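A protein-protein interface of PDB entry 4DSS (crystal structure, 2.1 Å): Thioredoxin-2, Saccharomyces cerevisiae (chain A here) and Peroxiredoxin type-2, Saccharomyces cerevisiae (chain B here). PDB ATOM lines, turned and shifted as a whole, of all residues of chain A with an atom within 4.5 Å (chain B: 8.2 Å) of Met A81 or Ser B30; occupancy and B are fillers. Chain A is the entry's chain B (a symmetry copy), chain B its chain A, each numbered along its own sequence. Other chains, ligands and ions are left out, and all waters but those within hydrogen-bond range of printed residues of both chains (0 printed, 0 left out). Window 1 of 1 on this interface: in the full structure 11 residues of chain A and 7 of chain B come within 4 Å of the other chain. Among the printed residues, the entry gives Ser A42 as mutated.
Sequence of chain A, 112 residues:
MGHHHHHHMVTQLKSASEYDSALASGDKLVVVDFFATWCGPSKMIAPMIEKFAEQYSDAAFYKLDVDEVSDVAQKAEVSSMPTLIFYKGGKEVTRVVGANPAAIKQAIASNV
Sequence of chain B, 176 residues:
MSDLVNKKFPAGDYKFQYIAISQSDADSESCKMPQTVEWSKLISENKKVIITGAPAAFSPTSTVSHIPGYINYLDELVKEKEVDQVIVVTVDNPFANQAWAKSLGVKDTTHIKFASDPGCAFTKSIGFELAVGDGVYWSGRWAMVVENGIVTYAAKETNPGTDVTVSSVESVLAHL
OG of Ser B30 lies within hydrogen-bond range of OG of Ser A80, at 2.7 Å. SG of Cys B31 is disulfide-bonded to SG of Cys A39 (2.1 Å). N of Cys B31 is in hydrogen-bond range of O of Met A81, 2.8 Å away.
N of Ser A42 sits at hydrogen-bond distance from SG of Cys A39. O of Ser A80 lies within hydrogen-bond range of OG1 of Thr A83, 2.6 Å away. The side-chain hydroxyl (OG) of Ser B30 lies within hydrogen-bond range of the side-chain amino group (NZ) of Lys B32. The backbone NH (N) of Gly A98 lies within hydrogen-bond range of the backbone carbonyl oxygen (O) of Pro A82 (2.7 Å).
CB of Cys B31 touches CZ3 of Trp A38 (3.4 Å). CG of Glu B29 touches CG of Pro A41, 3.2 Å away. CG of Pro A41 touches N of Ser B30 (3.95 Å). CD of Pro A41 touches SG of Cys B31 (3.6 Å). Ser A80 touches Cys B31 (CA to O, 3.4 Å). O of Met A81 touches CA of Ser B30, 3.2 Å away. Met A81 touches Met B33 (CE to CG, 3.5 Å). Ser B28 touches Gly A98. Glu B29 touches Gly A98.
Met A81 touches just these residues of chain B: Ser B30, Cys B31 and Met B33. Of the printed residues of chain A, Ser B30 touches Pro A41, Ser A80 and Met A81. Of chain B, only Ser B30 (2.7 Å) and Cys B31 (3.4 Å) come within 4 Å of Ser A80. Of the printed residues of chain B, Trp A38 touches Cys B31 (3.4 Å). Of the printed residues of chain B, Pro A41 touches Glu B29, Ser B30 and Cys B31. Printed residues of chain B within 4 Å of Gly A98: Ser B28 (3.9 Å) and Glu B29 (3.5 Å). Ser A42 touches none of the printed residues of chain B. The nearest residue of chain B that does not touch Met A81 is Glu B29 (4.7 Å). The nearest printed residue of chain B that does not touch Trp A38 is Lys B32 (4.5 Å).
Of the 15 printed residues of chain B, 5 touch a printed residue of chain A. Hydrophobic or aromatic side chains of chain B within 4 Å of the printed part of chain A: Met B33. Along chain B the printed residues that touch a printed residue of chain A span positions 28 to 33. Of the 14 printed residues of chain A, 6 touch a printed residue of chain B. Printed residues of chain A that touch a printed residue of chain B: Trp A38, Cys A39, Pro A41, Ser A80, Met A81 and Gly A98. Among the printed residues, 12 pairs touch across the chains.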
ATOM      1  N   PHE A  34     -22.243  15.487   5.352  1.00  0.00           N
ATOM      2  CA  PHE A  34     -21.266  14.884   6.237  1.00  0.00           C
ATOM      3  C   PHE A  34     -20.739  15.949   7.195  1.00  0.00           C
ATOM      4  O   PHE A  34     -20.071  16.899   6.776  1.00  0.00           O
ATOM      5  CB  PHE A  34     -20.137  14.255   5.419  1.00  0.00           C
ATOM      6  CG  PHE A  34     -20.564  13.042   4.632  1.00  0.00           C
ATOM      7  CD1 PHE A  34     -21.266  13.177   3.433  1.00  0.00           C
ATOM      8  CD2 PHE A  34     -20.260  11.755   5.089  1.00  0.00           C
ATOM      9  CE1 PHE A  34     -21.656  12.050   2.705  1.00  0.00           C
ATOM     10  CE2 PHE A  34     -20.648  10.632   4.371  1.00  0.00           C
ATOM     11  CZ  PHE A  34     -21.349  10.777   3.178  1.00  0.00           C
ATOM     12  N   PHE A  35     -21.060  15.793   8.476  1.00  0.00           N
ATOM     13  CA  PHE A  35     -20.800  16.836   9.474  1.00  0.00           C
ATOM     14  C   PHE A  35     -20.059  16.291  10.689  1.00  0.00           C
ATOM     15  O   PHE A  35     -19.937  15.080  10.853  1.00  0.00           O
ATOM     16  CB  PHE A  35     -22.115  17.535   9.903  1.00  0.00           C
ATOM     17  CG  PHE A  35     -22.986  16.711  10.838  1.00  0.00           C
ATOM     18  CD1 PHE A  35     -22.921  16.903  12.222  1.00  0.00           C
ATOM     19  CD2 PHE A  35     -23.881  15.765  10.335  1.00  0.00           C
ATOM     20  CE1 PHE A  35     -23.723  16.141  13.101  1.00  0.00           C
ATOM     21  CE2 PHE A  35     -24.686  15.002  11.200  1.00  0.00           C
ATOM     22  CZ  PHE A  35     -24.602  15.192  12.588  1.00  0.00           C
ATOM     23  N   ALA A  36     -19.554  17.195  11.522  1.00  0.00           N
ATOM     24  CA  ALA A  36     -19.001  16.830  12.830  1.00  0.00           C
ATOM     25  C   ALA A  36     -19.572  17.786  13.875  1.00  0.00           C
ATOM     26  O   ALA A  36     -19.691  18.972  13.613  1.00  0.00           O
ATOM     27  CB  ALA A  36     -17.481  16.902  12.812  1.00  0.00           C
ATOM     28  N   TRP A  38     -18.294  18.926  16.570  1.00  0.00           N
ATOM     29  CA  TRP A  38     -17.280  19.843  17.101  1.00  0.00           C
ATOM     30  C   TRP A  38     -16.856  20.904  16.088  1.00  0.00           C
ATOM     31  O   TRP A  38     -16.055  21.791  16.402  1.00  0.00           O
ATOM     32  CB  TRP A  38     -16.052  19.043  17.531  1.00  0.00           C
ATOM     33  CG  TRP A  38     -15.564  18.052  16.486  1.00  0.00           C
ATOM     34  CD1 TRP A  38     -15.825  16.711  16.446  1.00  0.00           C
ATOM     35  CD2 TRP A  38     -14.728  18.331  15.349  1.00  0.00           C
ATOM     36  NE1 TRP A  38     -15.201  16.135  15.361  1.00  0.00           N
ATOM     37  CE2 TRP A  38     -14.518  17.106  14.674  1.00  0.00           C
ATOM     38  CE3 TRP A  38     -14.125  19.490  14.848  1.00  0.00           C
ATOM     39  CZ2 TRP A  38     -13.745  17.011  13.510  1.00  0.00           C
ATOM     40  CZ3 TRP A  38     -13.349  19.395  13.690  1.00  0.00           C
ATOM     41  CH2 TRP A  38     -13.168  18.160  13.036  1.00  0.00           C
ATOM     42  N   CYS A  39     -17.385  20.799  14.871  1.00  0.00           N
ATOM     43  CA  CYS A  39     -16.922  21.594  13.737  1.00  0.00           C
ATOM     44  C   CYS A  39     -17.716  22.886  13.596  1.00  0.00           C
ATOM     45  O   CYS A  39     -18.929  22.845  13.401  1.00  0.00           O
ATOM     46  CB  CYS A  39     -17.022  20.754  12.456  1.00  0.00           C
ATOM     47  SG  CYS A  39     -16.650  21.632  10.919  1.00  0.00           S
ATOM     48  N   PRO A  41     -17.830  25.324  11.113  1.00  0.00           N
ATOM     49  CA  PRO A  41     -18.509  25.412   9.816  1.00  0.00           C
ATOM     50  C   PRO A  41     -19.668  24.428   9.627  1.00  0.00           C
ATOM     51  O   PRO A  41     -20.622  24.751   8.915  1.00  0.00           O
ATOM     52  CB  PRO A  41     -17.393  25.108   8.817  1.00  0.00           C
ATOM     53  CG  PRO A  41     -16.160  25.504   9.501  1.00  0.00           C
ATOM     54  CD  PRO A  41     -16.366  25.237  10.956  1.00  0.00           C
ATOM     55  N   SER A  42     -19.582  23.243  10.237  1.00  0.00           N
ATOM     56  CA  SER A  42     -20.713  22.297  10.232  1.00  0.00           C
ATOM     57  C   SER A  42     -21.927  22.874  10.948  1.00  0.00           C
ATOM     58  O   SER A  42     -23.036  22.834  10.418  1.00  0.00           O
ATOM     59  CB  SER A  42     -20.337  20.962  10.882  1.00  0.00           C
ATOM     60  OG  SER A  42     -19.677  20.111   9.966  1.00  0.00           O
ATOM     61  N   VAL A  66     -19.653  12.177  10.871  1.00  0.00           N
ATOM     62  CA  VAL A  66     -18.436  11.477  10.436  1.00  0.00           C
ATOM     63  C   VAL A  66     -17.699  10.725  11.551  1.00  0.00           C
ATOM     64  O   VAL A  66     -16.974   9.782  11.268  1.00  0.00           O
ATOM     65  CB  VAL A  66     -17.448  12.421   9.684  1.00  0.00           C
ATOM     66  CG1 VAL A  66     -18.113  13.003   8.433  1.00  0.00           C
ATOM     67  CG2 VAL A  66     -16.948  13.535  10.599  1.00  0.00           C
ATOM     68  N   VAL A  78     -14.515  11.464   2.257  1.00  0.00           N
ATOM     69  CA  VAL A  78     -14.757  12.722   2.941  1.00  0.00           C
ATOM     70  C   VAL A  78     -13.564  12.910   3.865  1.00  0.00           C
ATOM     71  O   VAL A  78     -13.304  12.067   4.724  1.00  0.00           O
ATOM     72  CB  VAL A  78     -16.068  12.670   3.767  1.00  0.00           C
ATOM     73  CG1 VAL A  78     -16.189  13.881   4.688  1.00  0.00           C
ATOM     74  CG2 VAL A  78     -17.282  12.546   2.858  1.00  0.00           C
ATOM     75  N   SER A  80     -13.031  16.243   4.950  1.00  0.00           N
ATOM     76  CA  SER A  80     -13.303  17.621   5.307  1.00  0.00           C
ATOM     77  C   SER A  80     -14.787  17.799   5.586  1.00  0.00           C
ATOM     78  O   SER A  80     -15.615  17.175   4.930  1.00  0.00           O
ATOM     79  CB  SER A  80     -12.889  18.526   4.148  1.00  0.00           C
ATOM     80  OG  SER A  80     -13.181  19.868   4.442  1.00  0.00           O
ATOM     81  N   MET A  81     -15.118  18.645   6.562  1.00  0.00           N
ATOM     82  CA  MET A  81     -16.518  18.910   6.914  1.00  0.00           C
ATOM     83  C   MET A  81     -16.810  20.407   7.024  1.00  0.00           C
ATOM     84  O   MET A  81     -16.032  21.139   7.639  1.00  0.00           O
ATOM     85  CB  MET A  81     -16.893  18.229   8.236  1.00  0.00           C
ATOM     86  CG  MET A  81     -16.844  16.705   8.216  1.00  0.00           C
ATOM     87  SD  MET A  81     -15.169  16.027   8.359  1.00  0.00           S
ATOM     88  CE  MET A  81     -14.686  16.549  10.011  1.00  0.00           C
ATOM     89  N   PRO A  82     -17.955  20.861   6.476  1.00  0.00           N
ATOM     90  CA  PRO A  82     -18.963  20.033   5.819  1.00  0.00           C
ATOM     91  C   PRO A  82     -18.558  19.599   4.414  1.00  0.00           C
ATOM     92  O   PRO A  82     -17.856  20.326   3.718  1.00  0.00           O
ATOM     93  CB  PRO A  82     -20.188  20.965   5.732  1.00  0.00           C
ATOM     94  CG  PRO A  82     -19.650  22.335   5.768  1.00  0.00           C
ATOM     95  CD  PRO A  82     -18.362  22.282   6.548  1.00  0.00           C
ATOM     96  N   THR A  83     -18.966  18.394   4.035  1.00  0.00           N
ATOM     97  CA  THR A  83     -18.964  17.974   2.645  1.00  0.00           C
ATOM     98  C   THR A  83     -20.385  17.512   2.351  1.00  0.00           C
ATOM     99  O   THR A  83     -20.937  16.663   3.061  1.00  0.00           O
ATOM    100  CB  THR A  83     -17.958  16.828   2.363  1.00  0.00           C
ATOM    101  OG1 THR A  83     -16.617  17.284   2.581  1.00  0.00           O
ATOM    102  CG2 THR A  83     -18.084  16.328   0.926  1.00  0.00           C
ATOM    103  N   GLY A  98     -17.088  22.335   2.047  1.00  0.00           N
ATOM    104  CA  GLY A  98     -17.035  23.607   2.772  1.00  0.00           C
ATOM    105  C   GLY A  98     -18.398  24.236   2.989  1.00  0.00           C
ATOM    106  O   GLY A  98     -19.377  23.838   2.365  1.00  0.00           O
ATOM    107  N   ALA B  20      -4.509  17.673   5.964  1.00  0.00           N
ATOM    108  CA  ALA B  20      -4.296  18.742   4.997  1.00  0.00           C
ATOM    109  C   ALA B  20      -4.351  20.107   5.677  1.00  0.00           C
ATOM    110  O   ALA B  20      -5.041  20.277   6.687  1.00  0.00           O
ATOM    111  CB  ALA B  20      -5.347  18.668   3.869  1.00  0.00           C
ATOM    112  N   SER B  22      -4.648  24.210   4.028  1.00  0.00           N
ATOM    113  CA  SER B  22      -4.730  24.969   2.788  1.00  0.00           C
ATOM    114  C   SER B  22      -5.174  26.411   2.994  1.00  0.00           C
ATOM    115  O   SER B  22      -5.739  26.760   4.024  1.00  0.00           O
ATOM    116  CB  SER B  22      -5.665  24.271   1.803  1.00  0.00           C
ATOM    117  OG  SER B  22      -6.974  24.274   2.306  1.00  0.00           O
ATOM    118  N   SER B  24      -6.924  27.772   0.286  1.00  0.00           N
ATOM    119  CA  SER B  24      -8.113  27.782  -0.578  1.00  0.00           C
ATOM    120  C   SER B  24      -9.244  26.856  -0.103  1.00  0.00           C
ATOM    121  O   SER B  24     -10.379  26.979  -0.560  1.00  0.00           O
ATOM    122  CB  SER B  24      -7.758  27.481  -2.034  1.00  0.00           C
ATOM    123  OG  SER B  24      -7.372  26.128  -2.203  1.00  0.00           O
ATOM    124  N   ASP B  25      -8.934  25.911   0.783  1.00  0.00           N
ATOM    125  CA  ASP B  25      -9.991  25.229   1.538  1.00  0.00           C
ATOM    126  C   ASP B  25     -10.106  25.849   2.933  1.00  0.00           C
ATOM    127  O   ASP B  25     -10.651  25.257   3.867  1.00  0.00           O
ATOM    128  CB  ASP B  25      -9.819  23.700   1.562  1.00  0.00           C
ATOM    129  CG  ASP B  25     -10.756  22.985   0.581  1.00  0.00           C
ATOM    130  OD1 ASP B  25     -11.775  23.583   0.160  1.00  0.00           O
ATOM    131  OD2 ASP B  25     -10.477  21.816   0.238  1.00  0.00           O
ATOM    132  N   ALA B  26      -9.544  27.050   3.047  1.00  0.00           N
ATOM    133  CA  ALA B  26      -9.954  28.021   4.038  1.00  0.00           C
ATOM    134  C   ALA B  26     -10.990  28.890   3.326  1.00  0.00           C
ATOM    135  O   ALA B  26     -11.945  29.364   3.949  1.00  0.00           O
ATOM    136  CB  ALA B  26      -8.768  28.850   4.501  1.00  0.00           C
ATOM    137  N   ASP B  27     -10.796  29.069   2.013  1.00  0.00           N
ATOM    138  CA  ASP B  27     -11.757  29.748   1.118  1.00  0.00           C
ATOM    139  C   ASP B  27     -13.161  29.133   1.154  1.00  0.00           C
ATOM    140  O   ASP B  27     -14.174  29.838   1.014  1.00  0.00           O
ATOM    141  CB  ASP B  27     -11.200  29.851  -0.316  1.00  0.00           C
ATOM    142  CG  ASP B  27     -12.219  29.462  -1.383  1.00  0.00           C
ATOM    143  OD1 ASP B  27     -12.834  30.370  -1.983  1.00  0.00           O
ATOM    144  OD2 ASP B  27     -12.402  28.246  -1.618  1.00  0.00           O
ATOM    145  N   SER B  28     -13.203  27.814   1.311  1.00  0.00           N
ATOM    146  CA  SER B  28     -14.412  27.127   1.725  1.00  0.00           C
ATOM    147  C   SER B  28     -14.141  26.603   3.131  1.00  0.00           C
ATOM    148  O   SER B  28     -13.526  25.539   3.299  1.00  0.00           O
ATOM    149  CB  SER B  28     -14.760  25.992   0.761  1.00  0.00           C
ATOM    150  OG  SER B  28     -15.542  26.458  -0.324  1.00  0.00           O
ATOM    151  N   GLU B  29     -14.498  27.388   4.143  1.00  0.00           N
ATOM    152  CA  GLU B  29     -14.214  27.033   5.532  1.00  0.00           C
ATOM    153  C   GLU B  29     -14.780  25.657   5.815  1.00  0.00           C
ATOM    154  O   GLU B  29     -15.936  25.360   5.552  1.00  0.00           O
ATOM    155  CB  GLU B  29     -14.722  28.090   6.524  1.00  0.00           C
ATOM    156  CG  GLU B  29     -14.510  27.864   8.019  1.00  0.00           C
ATOM    157  CD  GLU B  29     -13.059  27.997   8.534  1.00  0.00           C
ATOM    158  OE1 GLU B  29     -12.565  27.062   9.194  1.00  0.00           O
ATOM    159  OE2 GLU B  29     -12.418  29.031   8.339  1.00  0.00           O
ATOM    160  N   SER B  30     -13.890  24.836   6.338  1.00  0.00           N
ATOM    161  CA  SER B  30     -14.120  23.425   6.615  1.00  0.00           C
ATOM    162  C   SER B  30     -13.079  22.923   7.611  1.00  0.00           C
ATOM    163  O   SER B  30     -11.942  23.401   7.625  1.00  0.00           O
ATOM    164  CB  SER B  30     -14.027  22.605   5.323  1.00  0.00           C
ATOM    165  OG  SER B  30     -12.683  22.492   4.878  1.00  0.00           O
ATOM    166  N   CYS B  31     -13.474  21.960   8.439  1.00  0.00           N
ATOM    167  CA  CYS B  31     -12.561  21.339   9.387  1.00  0.00           C
ATOM    168  C   CYS B  31     -12.020  20.060   8.778  1.00  0.00           C
ATOM    169  O   CYS B  31     -12.767  19.258   8.221  1.00  0.00           O
ATOM    170  CB  CYS B  31     -13.276  21.022  10.694  1.00  0.00           C
ATOM    171  SG  CYS B  31     -14.645  22.129  11.096  1.00  0.00           S
ATOM    172  N   LYS B  32     -10.716  19.868   8.901  1.00  0.00           N
ATOM    173  CA  LYS B  32     -10.031  18.788   8.214  1.00  0.00           C
ATOM    174  C   LYS B  32      -9.835  17.550   9.092  1.00  0.00           C
ATOM    175  O   LYS B  32      -9.658  17.659  10.297  1.00  0.00           O
ATOM    176  CB  LYS B  32      -8.691  19.282   7.667  1.00  0.00           C
ATOM    177  CG  LYS B  32      -8.779  19.978   6.316  1.00  0.00           C
ATOM    178  CD  LYS B  32      -9.039  21.462   6.471  1.00  0.00           C
ATOM    179  CE  LYS B  32      -8.941  22.174   5.146  1.00  0.00           C
ATOM    180  NZ  LYS B  32      -9.489  23.538   5.278  1.00  0.00           N
ATOM    181  N   MET B  33      -9.883  16.383   8.451  1.00  0.00           N
ATOM    182  CA  MET B  33      -9.714  15.076   9.081  1.00  0.00           C
ATOM    183  C   MET B  33      -8.454  14.402   8.561  1.00  0.00           C
ATOM    184  O   MET B  33      -8.029  14.697   7.442  1.00  0.00           O
ATOM    185  CB  MET B  33     -10.871  14.163   8.689  1.00  0.00           C
ATOM    186  CG  MET B  33     -12.095  14.309   9.504  1.00  0.00           C
ATOM    187  SD  MET B  33     -13.057  12.807   9.378  1.00  0.00           S
ATOM    188  CE  MET B  33     -12.484  11.976  10.871  1.00  0.00           C
ATOM    189  N   PRO B  34      -7.876  13.461   9.347  1.00  0.00           N
ATOM    190  CA  PRO B  34      -6.723  12.705   8.836  1.00  0.00           C
ATOM    191  C   PRO B  34      -7.066  11.884   7.599  1.00  0.00           C
ATOM    192  O   PRO B  34      -8.170  11.356   7.495  1.00  0.00           O
ATOM    193  CB  PRO B  34      -6.363  11.780  10.007  1.00  0.00           C
ATOM    194  CG  PRO B  34      -6.828  12.523  11.218  1.00  0.00           C
ATOM    195  CD  PRO B  34      -8.149  13.126  10.761  1.00  0.00           C
ATOM    196  N   GLN B  98      -0.201  18.204  12.835  1.00  0.00           N
ATOM    197  CA  GLN B  98      -0.798  19.337  12.122  1.00  0.00           C
ATOM    198  C   GLN B  98      -0.634  20.625  12.923  1.00  0.00           C
ATOM    199  O   GLN B  98      -0.318  21.684  12.360  1.00  0.00           O
ATOM    200  CB  GLN B  98      -2.282  19.104  11.820  1.00  0.00           C
ATOM    201  CG  GLN B  98      -2.865  20.160  10.884  1.00  0.00           C
ATOM    202  CD  GLN B  98      -4.352  20.340  11.026  1.00  0.00           C
ATOM    203  OE1 GLN B  98      -4.920  20.183  12.110  1.00  0.00           O
ATOM    204  NE2 GLN B  98      -5.001  20.685   9.928  1.00  0.00           N
ATOM    205  N   LYS B 102       1.536  23.926  11.762  1.00  0.00           N
ATOM    206  CA  LYS B 102       0.990  25.278  11.835  1.00  0.00           C
ATOM    207  C   LYS B 102       1.848  26.203  12.685  1.00  0.00           C
ATOM    208  O   LYS B 102       2.065  27.359  12.314  1.00  0.00           O
ATOM    209  CB  LYS B 102      -0.442  25.285  12.375  1.00  0.00           C
ATOM    210  CG  LYS B 102      -1.501  24.823  11.383  1.00  0.00           C
ATOM    211  CD  LYS B 102      -2.875  24.937  12.027  1.00  0.00           C
ATOM    212  CE  LYS B 102      -3.907  24.049  11.343  1.00  0.00           C
ATOM    213  NZ  LYS B 102      -5.228  24.127  12.050  1.00  0.00           N
